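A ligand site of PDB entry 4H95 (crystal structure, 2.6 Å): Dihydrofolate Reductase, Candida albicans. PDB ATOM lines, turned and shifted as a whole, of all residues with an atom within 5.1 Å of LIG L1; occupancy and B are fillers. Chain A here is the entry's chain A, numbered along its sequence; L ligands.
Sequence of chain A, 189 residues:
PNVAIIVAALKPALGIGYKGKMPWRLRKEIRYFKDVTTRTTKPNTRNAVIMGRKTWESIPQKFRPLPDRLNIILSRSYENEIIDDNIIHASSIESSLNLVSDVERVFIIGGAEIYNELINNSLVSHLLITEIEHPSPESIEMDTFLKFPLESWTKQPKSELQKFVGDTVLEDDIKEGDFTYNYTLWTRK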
ATOM      1  N   ILE A   6      16.585  31.514  -5.290  1.00  0.00           N
ATOM      2  CA  ILE A   6      16.416  32.949  -5.503  1.00  0.00           C
ATOM      3  C   ILE A   6      15.256  33.208  -6.467  1.00  0.00           C
ATOM      4  O   ILE A   6      15.220  32.663  -7.581  1.00  0.00           O
ATOM      5  CB  ILE A   6      17.752  33.626  -5.965  1.00  0.00           C
ATOM      6  CG1 ILE A   6      17.593  35.153  -6.066  1.00  0.00           C
ATOM      7  CG2 ILE A   6      18.282  32.999  -7.254  1.00  0.00           C
ATOM      8  CD1 ILE A   6      18.910  35.915  -6.057  1.00  0.00           C
ATOM      9  N   VAL A   7      14.312  34.026  -6.025  1.00  0.00           N
ATOM     10  CA  VAL A   7      13.059  34.263  -6.760  1.00  0.00           C
ATOM     11  C   VAL A   7      12.432  35.611  -6.368  1.00  0.00           C
ATOM     12  O   VAL A   7      12.646  36.108  -5.269  1.00  0.00           O
ATOM     13  CB  VAL A   7      12.040  33.109  -6.523  1.00  0.00           C
ATOM     14  CG1 VAL A   7      11.639  32.997  -5.041  1.00  0.00           C
ATOM     15  CG2 VAL A   7      10.808  33.251  -7.426  1.00  0.00           C
ATOM     16  N   ALA A   8      11.677  36.199  -7.302  1.00  0.00           N
ATOM     17  CA  ALA A   8      10.855  37.374  -7.028  1.00  0.00           C
ATOM     18  C   ALA A   8       9.378  37.052  -7.264  1.00  0.00           C
ATOM     19  O   ALA A   8       8.991  36.655  -8.363  1.00  0.00           O
ATOM     20  CB  ALA A   8      11.296  38.548  -7.883  1.00  0.00           C
ATOM     21  N   ALA A   9       8.560  37.218  -6.229  1.00  0.00           N
ATOM     22  CA  ALA A   9       7.143  36.854  -6.288  1.00  0.00           C
ATOM     23  C   ALA A   9       6.235  37.948  -5.744  1.00  0.00           C
ATOM     24  O   ALA A   9       6.572  38.636  -4.790  1.00  0.00           O
ATOM     25  CB  ALA A   9       6.909  35.555  -5.540  1.00  0.00           C
ATOM     26  N   ILE A  16       4.403  34.250 -10.005  1.00  0.00           N
ATOM     27  CA  ILE A  16       5.713  34.478 -10.627  1.00  0.00           C
ATOM     28  C   ILE A  16       5.656  34.631 -12.150  1.00  0.00           C
ATOM     29  O   ILE A  16       6.671  34.947 -12.780  1.00  0.00           O
ATOM     30  CB  ILE A  16       6.744  33.386 -10.236  1.00  0.00           C
ATOM     31  CG1 ILE A  16       6.242  31.981 -10.603  1.00  0.00           C
ATOM     32  CG2 ILE A  16       7.108  33.487  -8.746  1.00  0.00           C
ATOM     33  CD1 ILE A  16       7.333  30.928 -10.655  1.00  0.00           C
ATOM     34  N   GLY A  17       4.476  34.415 -12.746  1.00  0.00           N
ATOM     35  CA  GLY A  17       4.322  34.559 -14.187  1.00  0.00           C
ATOM     36  C   GLY A  17       2.921  34.378 -14.743  1.00  0.00           C
ATOM     37  O   GLY A  17       2.020  33.893 -14.047  1.00  0.00           O
ATOM     38  N   TYR A  18       2.751  34.797 -15.996  1.00  0.00           N
ATOM     39  CA  TYR A  18       1.518  34.599 -16.753  1.00  0.00           C
ATOM     40  C   TYR A  18       1.857  34.346 -18.214  1.00  0.00           C
ATOM     41  O   TYR A  18       2.669  35.070 -18.797  1.00  0.00           O
ATOM     42  CB  TYR A  18       0.591  35.820 -16.605  1.00  0.00           C
ATOM     43  CG  TYR A  18      -0.646  35.774 -17.475  1.00  0.00           C
ATOM     44  CD1 TYR A  18      -1.727  34.936 -17.166  1.00  0.00           C
ATOM     45  CD2 TYR A  18      -0.759  36.595 -18.599  1.00  0.00           C
ATOM     46  CE1 TYR A  18      -2.871  34.903 -17.961  1.00  0.00           C
ATOM     47  CE2 TYR A  18      -1.896  36.573 -19.406  1.00  0.00           C
ATOM     48  CZ  TYR A  18      -2.952  35.723 -19.087  1.00  0.00           C
ATOM     49  OH  TYR A  18      -4.073  35.698 -19.879  1.00  0.00           O
ATOM     50  N   GLY A  20       3.695  32.173 -19.515  1.00  0.00           N
ATOM     51  CA  GLY A  20       5.113  31.845 -19.694  1.00  0.00           C
ATOM     52  C   GLY A  20       6.057  33.033 -19.686  1.00  0.00           C
ATOM     53  O   GLY A  20       7.154  32.950 -20.260  1.00  0.00           O
ATOM     54  N   LYS A  21       5.662  34.124 -19.042  1.00  0.00           N
ATOM     55  CA  LYS A  21       6.521  35.309 -18.925  1.00  0.00           C
ATOM     56  C   LYS A  21       6.289  36.103 -17.636  1.00  0.00           C
ATOM     57  O   LYS A  21       5.238  35.982 -17.009  1.00  0.00           O
ATOM     58  CB  LYS A  21       6.414  36.220 -20.166  1.00  0.00           C
ATOM     59  CG  LYS A  21       4.997  36.569 -20.606  1.00  0.00           C
ATOM     60  CD  LYS A  21       5.000  37.192 -21.989  1.00  0.00           C
ATOM     61  CE  LYS A  21       3.628  37.110 -22.658  1.00  0.00           C
ATOM     62  NZ  LYS A  21       2.599  37.956 -21.992  1.00  0.00           N
ATOM     63  N   MET A  22       7.283  36.905 -17.272  1.00  0.00           N
ATOM     64  CA  MET A  22       7.257  37.686 -16.035  1.00  0.00           C
ATOM     65  C   MET A  22       6.343  38.910 -16.153  1.00  0.00           C
ATOM     66  O   MET A  22       6.398  39.621 -17.157  1.00  0.00           O
ATOM     67  CB  MET A  22       8.671  38.109 -15.657  1.00  0.00           C
ATOM     68  CG  MET A  22       9.640  36.950 -15.451  1.00  0.00           C
ATOM     69  SD  MET A  22      11.223  37.428 -14.726  1.00  0.00           S
ATOM     70  CE  MET A  22      10.708  37.903 -13.078  1.00  0.00           C
ATOM     71  N   TRP A  24       6.418  41.720 -14.754  1.00  0.00           N
ATOM     72  CA  TRP A  24       7.101  42.961 -14.370  1.00  0.00           C
ATOM     73  C   TRP A  24       8.508  43.013 -14.944  1.00  0.00           C
ATOM     74  O   TRP A  24       9.113  41.987 -15.245  1.00  0.00           O
ATOM     75  CB  TRP A  24       7.171  43.089 -12.834  1.00  0.00           C
ATOM     76  CG  TRP A  24       7.606  41.819 -12.161  1.00  0.00           C
ATOM     77  CD1 TRP A  24       8.868  41.300 -12.117  1.00  0.00           C
ATOM     78  CD2 TRP A  24       6.769  40.909 -11.428  1.00  0.00           C
ATOM     79  NE1 TRP A  24       8.874  40.117 -11.410  1.00  0.00           N
ATOM     80  CE2 TRP A  24       7.596  39.859 -10.981  1.00  0.00           C
ATOM     81  CE3 TRP A  24       5.407  40.877 -11.120  1.00  0.00           C
ATOM     82  CZ2 TRP A  24       7.102  38.786 -10.229  1.00  0.00           C
ATOM     83  CZ3 TRP A  24       4.910  39.806 -10.377  1.00  0.00           C
ATOM     84  CH2 TRP A  24       5.765  38.776  -9.938  1.00  0.00           C
ATOM     85  N   MET A  51      18.779  25.912 -13.412  1.00  0.00           N
ATOM     86  CA  MET A  51      17.486  26.295 -13.972  1.00  0.00           C
ATOM     87  C   MET A  51      16.847  25.134 -14.730  1.00  0.00           C
ATOM     88  O   MET A  51      17.520  24.166 -15.102  1.00  0.00           O
ATOM     89  CB  MET A  51      17.651  27.494 -14.897  1.00  0.00           C
ATOM     90  CG  MET A  51      18.401  27.202 -16.191  1.00  0.00           C
ATOM     91  SD  MET A  51      18.941  28.698 -17.057  1.00  0.00           S
ATOM     92  CE  MET A  51      20.493  29.049 -16.224  1.00  0.00           C
ATOM     93  N   GLY A  52      15.535  25.226 -14.943  1.00  0.00           N
ATOM     94  CA  GLY A  52      14.816  24.310 -15.810  1.00  0.00           C
ATOM     95  C   GLY A  52      15.076  24.648 -17.260  1.00  0.00           C
ATOM     96  O   GLY A  52      15.527  25.742 -17.576  1.00  0.00           O
ATOM     97  N   ARG A  53      14.770  23.694 -18.146  1.00  0.00           N
ATOM     98  CA  ARG A  53      14.984  23.838 -19.581  1.00  0.00           C
ATOM     99  C   ARG A  53      14.201  25.014 -20.187  1.00  0.00           C
ATOM    100  O   ARG A  53      14.741  25.769 -20.994  1.00  0.00           O
ATOM    101  CB  ARG A  53      14.654  22.537 -20.325  1.00  0.00           C
ATOM    102  CG  ARG A  53      14.780  22.610 -21.848  1.00  0.00           C
ATOM    103  CD  ARG A  53      14.324  21.315 -22.529  1.00  0.00           C
ATOM    104  NE  ARG A  53      13.035  20.841 -22.026  1.00  0.00           N
ATOM    105  CZ  ARG A  53      11.852  21.260 -22.470  1.00  0.00           C
ATOM    106  NH1 ARG A  53      11.764  22.156 -23.448  1.00  0.00           N
ATOM    107  NH2 ARG A  53      10.735  20.763 -21.941  1.00  0.00           N
ATOM    108  N   LYS A  54      12.937  25.145 -19.789  1.00  0.00           N
ATOM    109  CA  LYS A  54      12.065  26.197 -20.294  1.00  0.00           C
ATOM    110  C   LYS A  54      12.585  27.583 -19.939  1.00  0.00           C
ATOM    111  O   LYS A  54      12.526  28.513 -20.759  1.00  0.00           O
ATOM    112  CB  LYS A  54      10.637  26.033 -19.777  1.00  0.00           C
ATOM    113  CG  LYS A  54       9.861  24.876 -20.392  1.00  0.00           C
ATOM    114  CD  LYS A  54       8.408  24.884 -19.931  1.00  0.00           C
ATOM    115  CE  LYS A  54       7.675  23.618 -20.332  1.00  0.00           C
ATOM    116  NZ  LYS A  54       6.328  23.541 -19.689  1.00  0.00           N
ATOM    117  N   THR A  55      13.089  27.721 -18.716  1.00  0.00           N
ATOM    118  CA  THR A  55      13.671  28.971 -18.235  1.00  0.00           C
ATOM    119  C   THR A  55      14.906  29.335 -19.043  1.00  0.00           C
ATOM    120  O   THR A  55      15.071  30.480 -19.454  1.00  0.00           O
ATOM    121  CB  THR A  55      13.994  28.877 -16.721  1.00  0.00           C
ATOM    122  OG1 THR A  55      12.768  28.698 -15.992  1.00  0.00           O
ATOM    123  CG2 THR A  55      14.688  30.140 -16.228  1.00  0.00           C
ATOM    124  N   LEU A  74      18.385  21.837 -16.448  1.00  0.00           N
ATOM    125  CA  LEU A  74      17.724  20.596 -16.043  1.00  0.00           C
ATOM    126  C   LEU A  74      16.674  20.147 -17.051  1.00  0.00           C
ATOM    127  O   LEU A  74      15.824  20.922 -17.486  1.00  0.00           O
ATOM    128  CB  LEU A  74      17.100  20.734 -14.654  1.00  0.00           C
ATOM    129  CG  LEU A  74      18.050  20.851 -13.449  1.00  0.00           C
ATOM    130  CD1 LEU A  74      17.258  20.903 -12.162  1.00  0.00           C
ATOM    131  CD2 LEU A  74      19.060  19.707 -13.409  1.00  0.00           C
ATOM    132  N   SER A  75      16.783  18.882 -17.417  1.00  0.00           N
ATOM    133  CA  SER A  75      15.780  18.216 -18.233  1.00  0.00           C
ATOM    134  C   SER A  75      15.779  16.759 -17.826  1.00  0.00           C
ATOM    135  O   SER A  75      16.833  16.197 -17.521  1.00  0.00           O
ATOM    136  CB  SER A  75      16.115  18.353 -19.718  1.00  0.00           C
ATOM    137  OG  SER A  75      15.330  17.469 -20.508  1.00  0.00           O
ATOM    138  N   ARG A  76      14.599  16.152 -17.839  1.00  0.00           N
ATOM    139  CA  ARG A  76      14.464  14.737 -17.524  1.00  0.00           C
ATOM    140  C   ARG A  76      14.967  13.866 -18.673  1.00  0.00           C
ATOM    141  O   ARG A  76      14.973  12.630 -18.566  1.00  0.00           O
ATOM    142  CB  ARG A  76      13.014  14.395 -17.150  1.00  0.00           C
ATOM    143  CG  ARG A  76      12.623  14.875 -15.758  1.00  0.00           C
ATOM    144  CD  ARG A  76      11.153  14.608 -15.461  1.00  0.00           C
ATOM    145  NE  ARG A  76      10.254  15.471 -16.231  1.00  0.00           N
ATOM    146  CZ  ARG A  76       9.656  16.559 -15.747  1.00  0.00           C
ATOM    147  NH1 ARG A  76       9.849  16.929 -14.488  1.00  0.00           N
ATOM    148  NH2 ARG A  76       8.852  17.267 -16.529  1.00  0.00           N
ATOM    149  N   SER A  77      15.392  14.509 -19.750  1.00  0.00           N
ATOM    150  CA  SER A  77      15.956  13.852 -20.928  1.00  0.00           C
ATOM    151  C   SER A  77      17.492  13.930 -20.958  1.00  0.00           C
ATOM    152  O   SER A  77      18.126  13.270 -21.770  1.00  0.00           O
ATOM    153  CB  SER A  77      15.408  14.497 -22.206  1.00  0.00           C
ATOM    154  OG  SER A  77      14.003  14.405 -22.252  1.00  0.00           O
ATOM    155  N   ALA A  90      22.069  18.268 -16.942  1.00  0.00           N
ATOM    156  CA  ALA A  90      21.827  17.303 -15.878  1.00  0.00           C
ATOM    157  C   ALA A  90      20.358  16.930 -15.743  1.00  0.00           C
ATOM    158  O   ALA A  90      19.475  17.661 -16.206  1.00  0.00           O
ATOM    159  CB  ALA A  90      22.378  17.816 -14.549  1.00  0.00           C
ATOM    160  N   SER A  91      20.093  15.791 -15.095  1.00  0.00           N
ATOM    161  CA  SER A  91      18.729  15.321 -14.834  1.00  0.00           C
ATOM    162  C   SER A  91      18.304  15.498 -13.375  1.00  0.00           C
ATOM    163  O   SER A  91      17.187  15.159 -13.003  1.00  0.00           O
ATOM    164  CB  SER A  91      18.562  13.871 -15.277  1.00  0.00           C
ATOM    165  OG  SER A  91      19.464  13.013 -14.606  1.00  0.00           O
ATOM    166  N   SER A  92      19.204  16.037 -12.553  1.00  0.00           N
ATOM    167  CA  SER A  92      18.917  16.337 -11.148  1.00  0.00           C
ATOM    168  C   SER A  92      19.977  17.261 -10.558  1.00  0.00           C
ATOM    169  O   SER A  92      21.108  17.313 -11.044  1.00  0.00           O
ATOM    170  CB  SER A  92      18.835  15.047 -10.317  1.00  0.00           C
ATOM    171  OG  SER A  92      20.125  14.550  -9.984  1.00  0.00           O
ATOM    172  N   ILE A 109      17.298  29.334  -9.946  1.00  0.00           N
ATOM    173  CA  ILE A 109      16.814  30.591 -10.525  1.00  0.00           C
ATOM    174  C   ILE A 109      15.528  30.450 -11.359  1.00  0.00           C
ATOM    175  O   ILE A 109      15.087  31.417 -11.976  1.00  0.00           O
ATOM    176  CB  ILE A 109      17.924  31.317 -11.335  1.00  0.00           C
ATOM    177  CG1 ILE A 109      18.265  30.547 -12.619  1.00  0.00           C
ATOM    178  CG2 ILE A 109      19.168  31.526 -10.471  1.00  0.00           C
ATOM    179  CD1 ILE A 109      19.104  31.335 -13.595  1.00  0.00           C
ATOM    180  N   GLY A 110      14.927  29.260 -11.341  1.00  0.00           N
ATOM    181  CA  GLY A 110      13.657  29.037 -12.055  1.00  0.00           C
ATOM    182  C   GLY A 110      13.597  27.741 -12.851  1.00  0.00           C
ATOM    183  O   GLY A 110      14.599  27.055 -13.007  1.00  0.00           O
ATOM    184  N   GLY A 111      12.404  27.387 -13.347  1.00  0.00           N
ATOM    185  CA  GLY A 111      11.184  28.167 -13.142  1.00  0.00           C
ATOM    186  C   GLY A 111      10.231  27.524 -12.149  1.00  0.00           C
ATOM    187  O   GLY A 111      10.652  26.914 -11.163  1.00  0.00           O
ATOM    188  N   ALA A 112       8.923  27.669 -12.430  1.00  0.00           N
ATOM    189  CA  ALA A 112       7.860  27.228 -11.519  1.00  0.00           C
ATOM    190  C   ALA A 112       7.934  25.757 -11.112  1.00  0.00           C
ATOM    191  O   ALA A 112       7.787  25.436  -9.922  1.00  0.00           O
ATOM    192  CB  ALA A 112       6.486  27.551 -12.124  1.00  0.00           C
ATOM    193  N   GLU A 113       8.169  24.867 -12.070  1.00  0.00           N
ATOM    194  CA  GLU A 113       8.279  23.435 -11.790  1.00  0.00           C
ATOM    195  C   GLU A 113       9.517  23.102 -10.958  1.00  0.00           C
ATOM    196  O   GLU A 113       9.472  22.248 -10.072  1.00  0.00           O
ATOM    197  CB  GLU A 113       8.258  22.616 -13.092  1.00  0.00           C
ATOM    198  CG  GLU A 113       8.174  21.102 -12.869  1.00  0.00           C
ATOM    199  CD  GLU A 113       7.811  20.325 -14.136  1.00  0.00           C
ATOM    200  OE1 GLU A 113       7.471  20.959 -15.161  1.00  0.00           O
ATOM    201  OE2 GLU A 113       7.848  19.077 -14.088  1.00  0.00           O
ATOM    202  N   ILE A 114      10.620  23.777 -11.273  1.00  0.00           N
ATOM    203  CA  ILE A 114      11.896  23.604 -10.558  1.00  0.00           C
ATOM    204  C   ILE A 114      11.792  24.123  -9.120  1.00  0.00           C
ATOM    205  O   ILE A 114      12.216  23.438  -8.182  1.00  0.00           O
ATOM    206  CB  ILE A 114      13.061  24.287 -11.312  1.00  0.00           C
ATOM    207  CG1 ILE A 114      13.178  23.757 -12.746  1.00  0.00           C
ATOM    208  CG2 ILE A 114      14.384  24.125 -10.559  1.00  0.00           C
ATOM    209  CD1 ILE A 114      13.723  22.326 -12.858  1.00  0.00           C
ATOM    210  N   TYR A 115      11.227  25.322  -8.956  1.00  0.00           N
ATOM    211  CA  TYR A 115      10.969  25.898  -7.632  1.00  0.00           C
ATOM    212  C   TYR A 115      10.121  24.977  -6.765  1.00  0.00           C
ATOM    213  O   TYR A 115      10.548  24.582  -5.675  1.00  0.00           O
ATOM    214  CB  TYR A 115      10.257  27.254  -7.751  1.00  0.00           C
ATOM    215  CG  TYR A 115      11.124  28.411  -8.210  1.00  0.00           C
ATOM    216  CD1 TYR A 115      12.404  28.624  -7.687  1.00  0.00           C
ATOM    217  CD2 TYR A 115      10.634  29.332  -9.144  1.00  0.00           C
ATOM    218  CE1 TYR A 115      13.182  29.698  -8.104  1.00  0.00           C
ATOM    219  CE2 TYR A 115      11.407  30.407  -9.570  1.00  0.00           C
ATOM    220  CZ  TYR A 115      12.677  30.591  -9.048  1.00  0.00           C
ATOM    221  OH  TYR A 115      13.444  31.655  -9.463  1.00  0.00           O
ATOM    222  N   GLU A 117       9.444  21.957  -6.706  1.00  0.00           N
ATOM    223  CA  GLU A 117      10.013  20.667  -6.320  1.00  0.00           C
ATOM    224  C   GLU A 117      11.172  20.822  -5.345  1.00  0.00           C
ATOM    225  O   GLU A 117      11.178  20.227  -4.266  1.00  0.00           O
ATOM    226  CB  GLU A 117      10.470  19.873  -7.557  1.00  0.00           C
ATOM    227  CG  GLU A 117       9.334  19.331  -8.406  1.00  0.00           C
ATOM    228  CD  GLU A 117       9.666  18.014  -9.078  1.00  0.00           C
ATOM    229  OE1 GLU A 117      10.839  17.839  -9.491  1.00  0.00           O
ATOM    230  OE2 GLU A 117       8.755  17.170  -9.210  1.00  0.00           O
ATOM    231  N   THR A 144       0.945  31.192 -13.027  1.00  0.00           N
ATOM    232  CA  THR A 144       1.918  30.339 -12.340  1.00  0.00           C
ATOM    233  C   THR A 144       2.269  30.882 -10.947  1.00  0.00           C
ATOM    234  O   THR A 144       2.603  32.058 -10.797  1.00  0.00           O
ATOM    235  CB  THR A 144       3.214  30.121 -13.149  1.00  0.00           C
ATOM    236  OG1 THR A 144       3.735  31.374 -13.583  1.00  0.00           O
ATOM    237  CG2 THR A 144       2.946  29.251 -14.372  1.00  0.00           C
HETATM  238  P1  LIG L   1      10.799  25.495 -15.833  1.00  0.00           P
HETATM  239  O1  LIG L   1      10.468  25.052 -14.461  1.00  0.00           O
HETATM  240  O2  LIG L   1      12.055  26.274 -15.840  1.00  0.00           O
HETATM  241  O3  LIG L   1      10.902  24.270 -16.866  1.00  0.00           O
HETATM  242  C1  LIG L   1      10.416  22.987 -16.561  1.00  0.00           C
HETATM  243  C2  LIG L   1      11.302  21.972 -17.267  1.00  0.00           C
HETATM  244  O4  LIG L   1      12.411  21.629 -16.462  1.00  0.00           O
HETATM  245  C3  LIG L   1      10.576  20.668 -17.569  1.00  0.00           C
HETATM  246  O5  LIG L   1      10.002  20.697 -18.853  1.00  0.00           O
HETATM  247  C4  LIG L   1      11.671  19.633 -17.477  1.00  0.00           C
HETATM  248  O6  LIG L   1      12.321  19.530 -18.717  1.00  0.00           O
HETATM  249  C5  LIG L   1      12.666  20.241 -16.494  1.00  0.00           C
HETATM  250  N1  LIG L   1      12.512  19.690 -15.136  1.00  0.00           N
HETATM  251  C6  LIG L   1      11.505  19.960 -14.247  1.00  0.00           C
HETATM  252  N2  LIG L   1      11.720  19.274 -13.106  1.00  0.00           N
HETATM  253  C7  LIG L   1      12.858  18.558 -13.245  1.00  0.00           C
HETATM  254  C8  LIG L   1      13.534  17.692 -12.386  1.00  0.00           C
HETATM  255  N3  LIG L   1      13.052  17.444 -11.169  1.00  0.00           N
HETATM  256  N4  LIG L   1      14.701  17.081 -12.802  1.00  0.00           N
HETATM  257  C9  LIG L   1      15.206  17.345 -14.069  1.00  0.00           C
HETATM  258  N5  LIG L   1      14.525  18.210 -14.914  1.00  0.00           N
HETATM  259  C10 LIG L   1      13.372  18.813 -14.517  1.00  0.00           C
HETATM  260  O7  LIG L   1       9.601  26.377 -16.437  1.00  0.00           O
HETATM  261  P2  LIG L   1       8.063  26.566 -15.995  1.00  0.00           P
HETATM  262  O8  LIG L   1       7.268  26.711 -17.235  1.00  0.00           O
HETATM  263  O9  LIG L   1       7.706  25.538 -15.006  1.00  0.00           O
HETATM  264  O10 LIG L   1       8.111  27.990 -15.226  1.00  0.00           O
HETATM  265  C11 LIG L   1       8.477  29.171 -15.917  1.00  0.00           C
HETATM  266  C12 LIG L   1       7.653  30.346 -15.403  1.00  0.00           C
HETATM  267  O11 LIG L   1       8.203  30.828 -14.189  1.00  0.00           O
HETATM  268  C13 LIG L   1       7.626  31.503 -16.379  1.00  0.00           C
HETATM  269  O12 LIG L   1       6.288  31.892 -16.593  1.00  0.00           O
HETATM  270  C14 LIG L   1       8.392  32.632 -15.711  1.00  0.00           C
HETATM  271  O13 LIG L   1       7.728  33.866 -15.850  1.00  0.00           O
HETATM  272  C15 LIG L   1       8.451  32.225 -14.247  1.00  0.00           C
HETATM  273  N6  LIG L   1       9.741  32.582 -13.614  1.00  0.00           N
HETATM  274  C16 LIG L   1       9.757  33.547 -12.644  1.00  0.00           C
HETATM  275  C17 LIG L   1      10.948  33.910 -12.014  1.00  0.00           C
HETATM  276  C18 LIG L   1      10.950  34.936 -10.917  1.00  0.00           C
HETATM  277  O14 LIG L   1      12.068  35.054 -10.074  1.00  0.00           O
HETATM  278  N7  LIG L   1       9.880  35.723 -10.738  1.00  0.00           N
HETATM  279  C19 LIG L   1      12.130  33.282 -12.394  1.00  0.00           C
HETATM  280  C20 LIG L   1      12.118  32.299 -13.381  1.00  0.00           C
HETATM  281  C21 LIG L   1      10.903  31.954 -13.987  1.00  0.00           C
HETATM  282  P3  LIG L   1      12.071  18.336 -19.768  1.00  0.00           P
HETATM  283  O15 LIG L   1      13.124  18.461 -20.853  1.00  0.00           O
HETATM  284  O16 LIG L   1      12.196  16.991 -19.095  1.00  0.00           O
HETATM  285  O17 LIG L   1      10.696  18.478 -20.384  1.00  0.00           O
HETATM  286  N1  LG2 L   2      15.077  35.725  -9.053  1.00  0.00           N
HETATM  287  C1  LG2 L   2      15.167  37.103  -8.887  1.00  0.00           C
HETATM  288  N2  LG2 L   2      15.261  37.933 -10.005  1.00  0.00           N
HETATM  289  C2  LG2 L   2      15.280  37.395 -11.304  1.00  0.00           C
HETATM  290  C3  LG2 L   2      15.198  36.013 -11.451  1.00  0.00           C
HETATM  291  C4  LG2 L   2      15.091  35.175 -10.340  1.00  0.00           C
HETATM  292  C5  LG2 L   2      18.881  37.818 -17.077  1.00  0.00           C
HETATM  293  N3  LG2 L   2      15.151  37.612  -7.661  1.00  0.00           N
HETATM  294  C6  LG2 L   2      15.411  38.375 -12.486  1.00  0.00           C
HETATM  295  N4  LG2 L   2      15.012  33.862 -10.476  1.00  0.00           N
HETATM  296  C7  LG2 L   2      15.206  35.426 -12.754  1.00  0.00           C
HETATM  297  C8  LG2 L   2      15.223  34.939 -13.868  1.00  0.00           C
HETATM  298  C9  LG2 L   2      15.235  34.315 -15.190  1.00  0.00           C
HETATM  299  C10 LG2 L   2      16.394  33.322 -15.258  1.00  0.00           C
HETATM  300  C11 LG2 L   2      15.383  35.383 -16.297  1.00  0.00           C
HETATM  301  C12 LG2 L   2      14.470  35.381 -17.353  1.00  0.00           C
HETATM  302  C13 LG2 L   2      14.568  36.336 -18.373  1.00  0.00           C
HETATM  303  C14 LG2 L   2      15.602  37.271 -18.339  1.00  0.00           C
HETATM  304  C15 LG2 L   2      16.525  37.283 -17.285  1.00  0.00           C
HETATM  305  C16 LG2 L   2      16.404  36.330 -16.266  1.00  0.00           C
HETATM  306  C17 LG2 L   2      17.555  38.221 -17.259  1.00  0.00           C
HETATM  307  C18 LG2 L   2      17.288  39.581 -17.425  1.00  0.00           C
HETATM  308  C19 LG2 L   2      18.360  40.486 -17.401  1.00  0.00           C
HETATM  309  N5  LG2 L   2      19.599  40.057 -17.221  1.00  0.00           N
HETATM  310  C20 LG2 L   2      19.895  38.778 -17.063  1.00  0.00           C
HETATM  311  C21 LG2 L   2      14.080  39.013 -12.863  1.00  0.00           C
HETATM  312  O1  LG2 L   2      13.681  36.341 -19.417  1.00  0.00           O
HETATM  313  C22 LG2 L   2      12.433  37.006 -19.123  1.00  0.00           C
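The backbone NH (N) of Ser 75 lies within hydrogen-bond range of a nitrogen (N5) of LIG L1 (3.4 Å). O15 of LIG L1 is in hydrogen-bond range of OG of Ser 75, at 2.4 Å. The backbone NH of Thr 55 lies close to an oxygen (O2) of LIG L1, 3.4 Å away. The side-chain hydroxyl (OG1) of Thr 55 is in hydrogen-bond range of an oxygen (O2) of LIG L1 (2.5 Å). NE of Arg 53 lies within salt-bridge range of O15 of LIG L1. An oxygen (O14) of LIG L1 is in hydrogen-bond range of the backbone NH (N) of Ala 8, at 3.0 Å. O of Ala 8 sits at hydrogen-bond distance from N7 of LIG L1 (2.7 Å). An oxygen (O2) of LIG L1 sits at hydrogen-bond distance from the backbone NH (N) of Gly 111 (2.8 Å). OE1 of Glu 117 lies within hydrogen-bond range of N3 of LIG L1 (2.8 Å). The backbone NH (N) of Arg 76 lies within hydrogen-bond range of an oxygen (O16) of LIG L1, at 2.8 Å. O16 of LIG L1 lies within salt-bridge range of NE of Arg 76. The backbone NH (N) of Ala 112 lies within hydrogen-bond range of an oxygen (O10) of LIG L1, 2.9 Å away. N of Glu 113 sits at hydrogen-bond distance from O9 of LIG L1 (3.0 Å). The backbone NH (N) of Lys 21 lies within hydrogen-bond range of an oxygen (O12) of LIG L1, at 3.4 Å. O of Lys 21 sits close to O13 of LIG L1 (3.5 Å). The backbone NH of Met 22 sits at hydrogen-bond distance from an oxygen (O13) of LIG L1 (3.4 Å). O of Ile 16 sits close to O13 of LIG L1, at 3.4 Å. O1 of LIG L1 is in hydrogen-bond range of N of Ile 114 (3.4 Å). A nitrogen (N4) of LG2 L2 sits at hydrogen-bond distance from the backbone carbonyl oxygen (O) of Ile 109 (2.9 Å). The side-chain hydroxyl of Tyr 115 sits at hydrogen-bond distance from a nitrogen (N4) of LG2 L2, at 2.9 Å. The backbone carbonyl oxygen (O) of Ile 6 is in hydrogen-bond range of a nitrogen (N4) of LG2 L2.
N4 of LG2 L2 lies close to O14 of LIG L1 (3.2 Å).
The side-chain hydroxyl of Ser 75 sits close to the backbone NH of Ser 77 (3.1 Å). N of Gly 111 sits at hydrogen-bond distance from OG1 of Thr 55, 3.0 Å away. The guanidinium group (NH1) of Arg 76 lies within salt-bridge range of the side-chain carboxylate (OE2) of Glu 113 (3.0 Å). The backbone NH (N) of Leu 74 sits at hydrogen-bond distance from the backbone carbonyl oxygen (O) of Met 51 (2.8 Å). N of Gly 52 is in hydrogen-bond range of O of Gly 110 (2.8 Å). The backbone carbonyl oxygen (O) of Thr 144 is in hydrogen-bond range of the backbone NH (N) of Ile 16, at 2.9 Å. O of Ile 109 is in hydrogen-bond range of OH of Tyr 115 (3.0 Å). The backbone carbonyl oxygen (O) of Gly 17 is in hydrogen-bond range of the backbone NH (N) of Thr 144, 3.1 Å away.
A nitrogen (N4) of LIG L1 sits close to the backbone carbonyl oxygen of Ser 91, at 3.1 Å. Residues that only touch LIG L1: Gly 20 (3.3 Å), Leu 74 (3.4 Å), Gly 52 (3.4 Å), Ile 109 (3.4 Å), Lys 54 (3.4 Å), Val 7 (3.4 Å), Tyr 115 (3.6 Å), Gly 110 (3.7 Å), Gly 17 (3.9 Å) and Thr 144 (3.98 Å). Within 4 Å of LIG L1: Val 7, Ala 8, Ile 16, Gly 17, Gly 20, Lys 21, Met 22, Gly 52, Arg 53, Lys 54, Thr 55, Leu 74, Ser 75, Arg 76, Ser 91, Ile 109, Gly 110, Gly 111, Ala 112, Glu 113, Ile 114, Tyr 115, Glu 117 and Thr 144. The nearest printed residue that does not touch LIG L1 is Ser 77 (4.1 Å).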
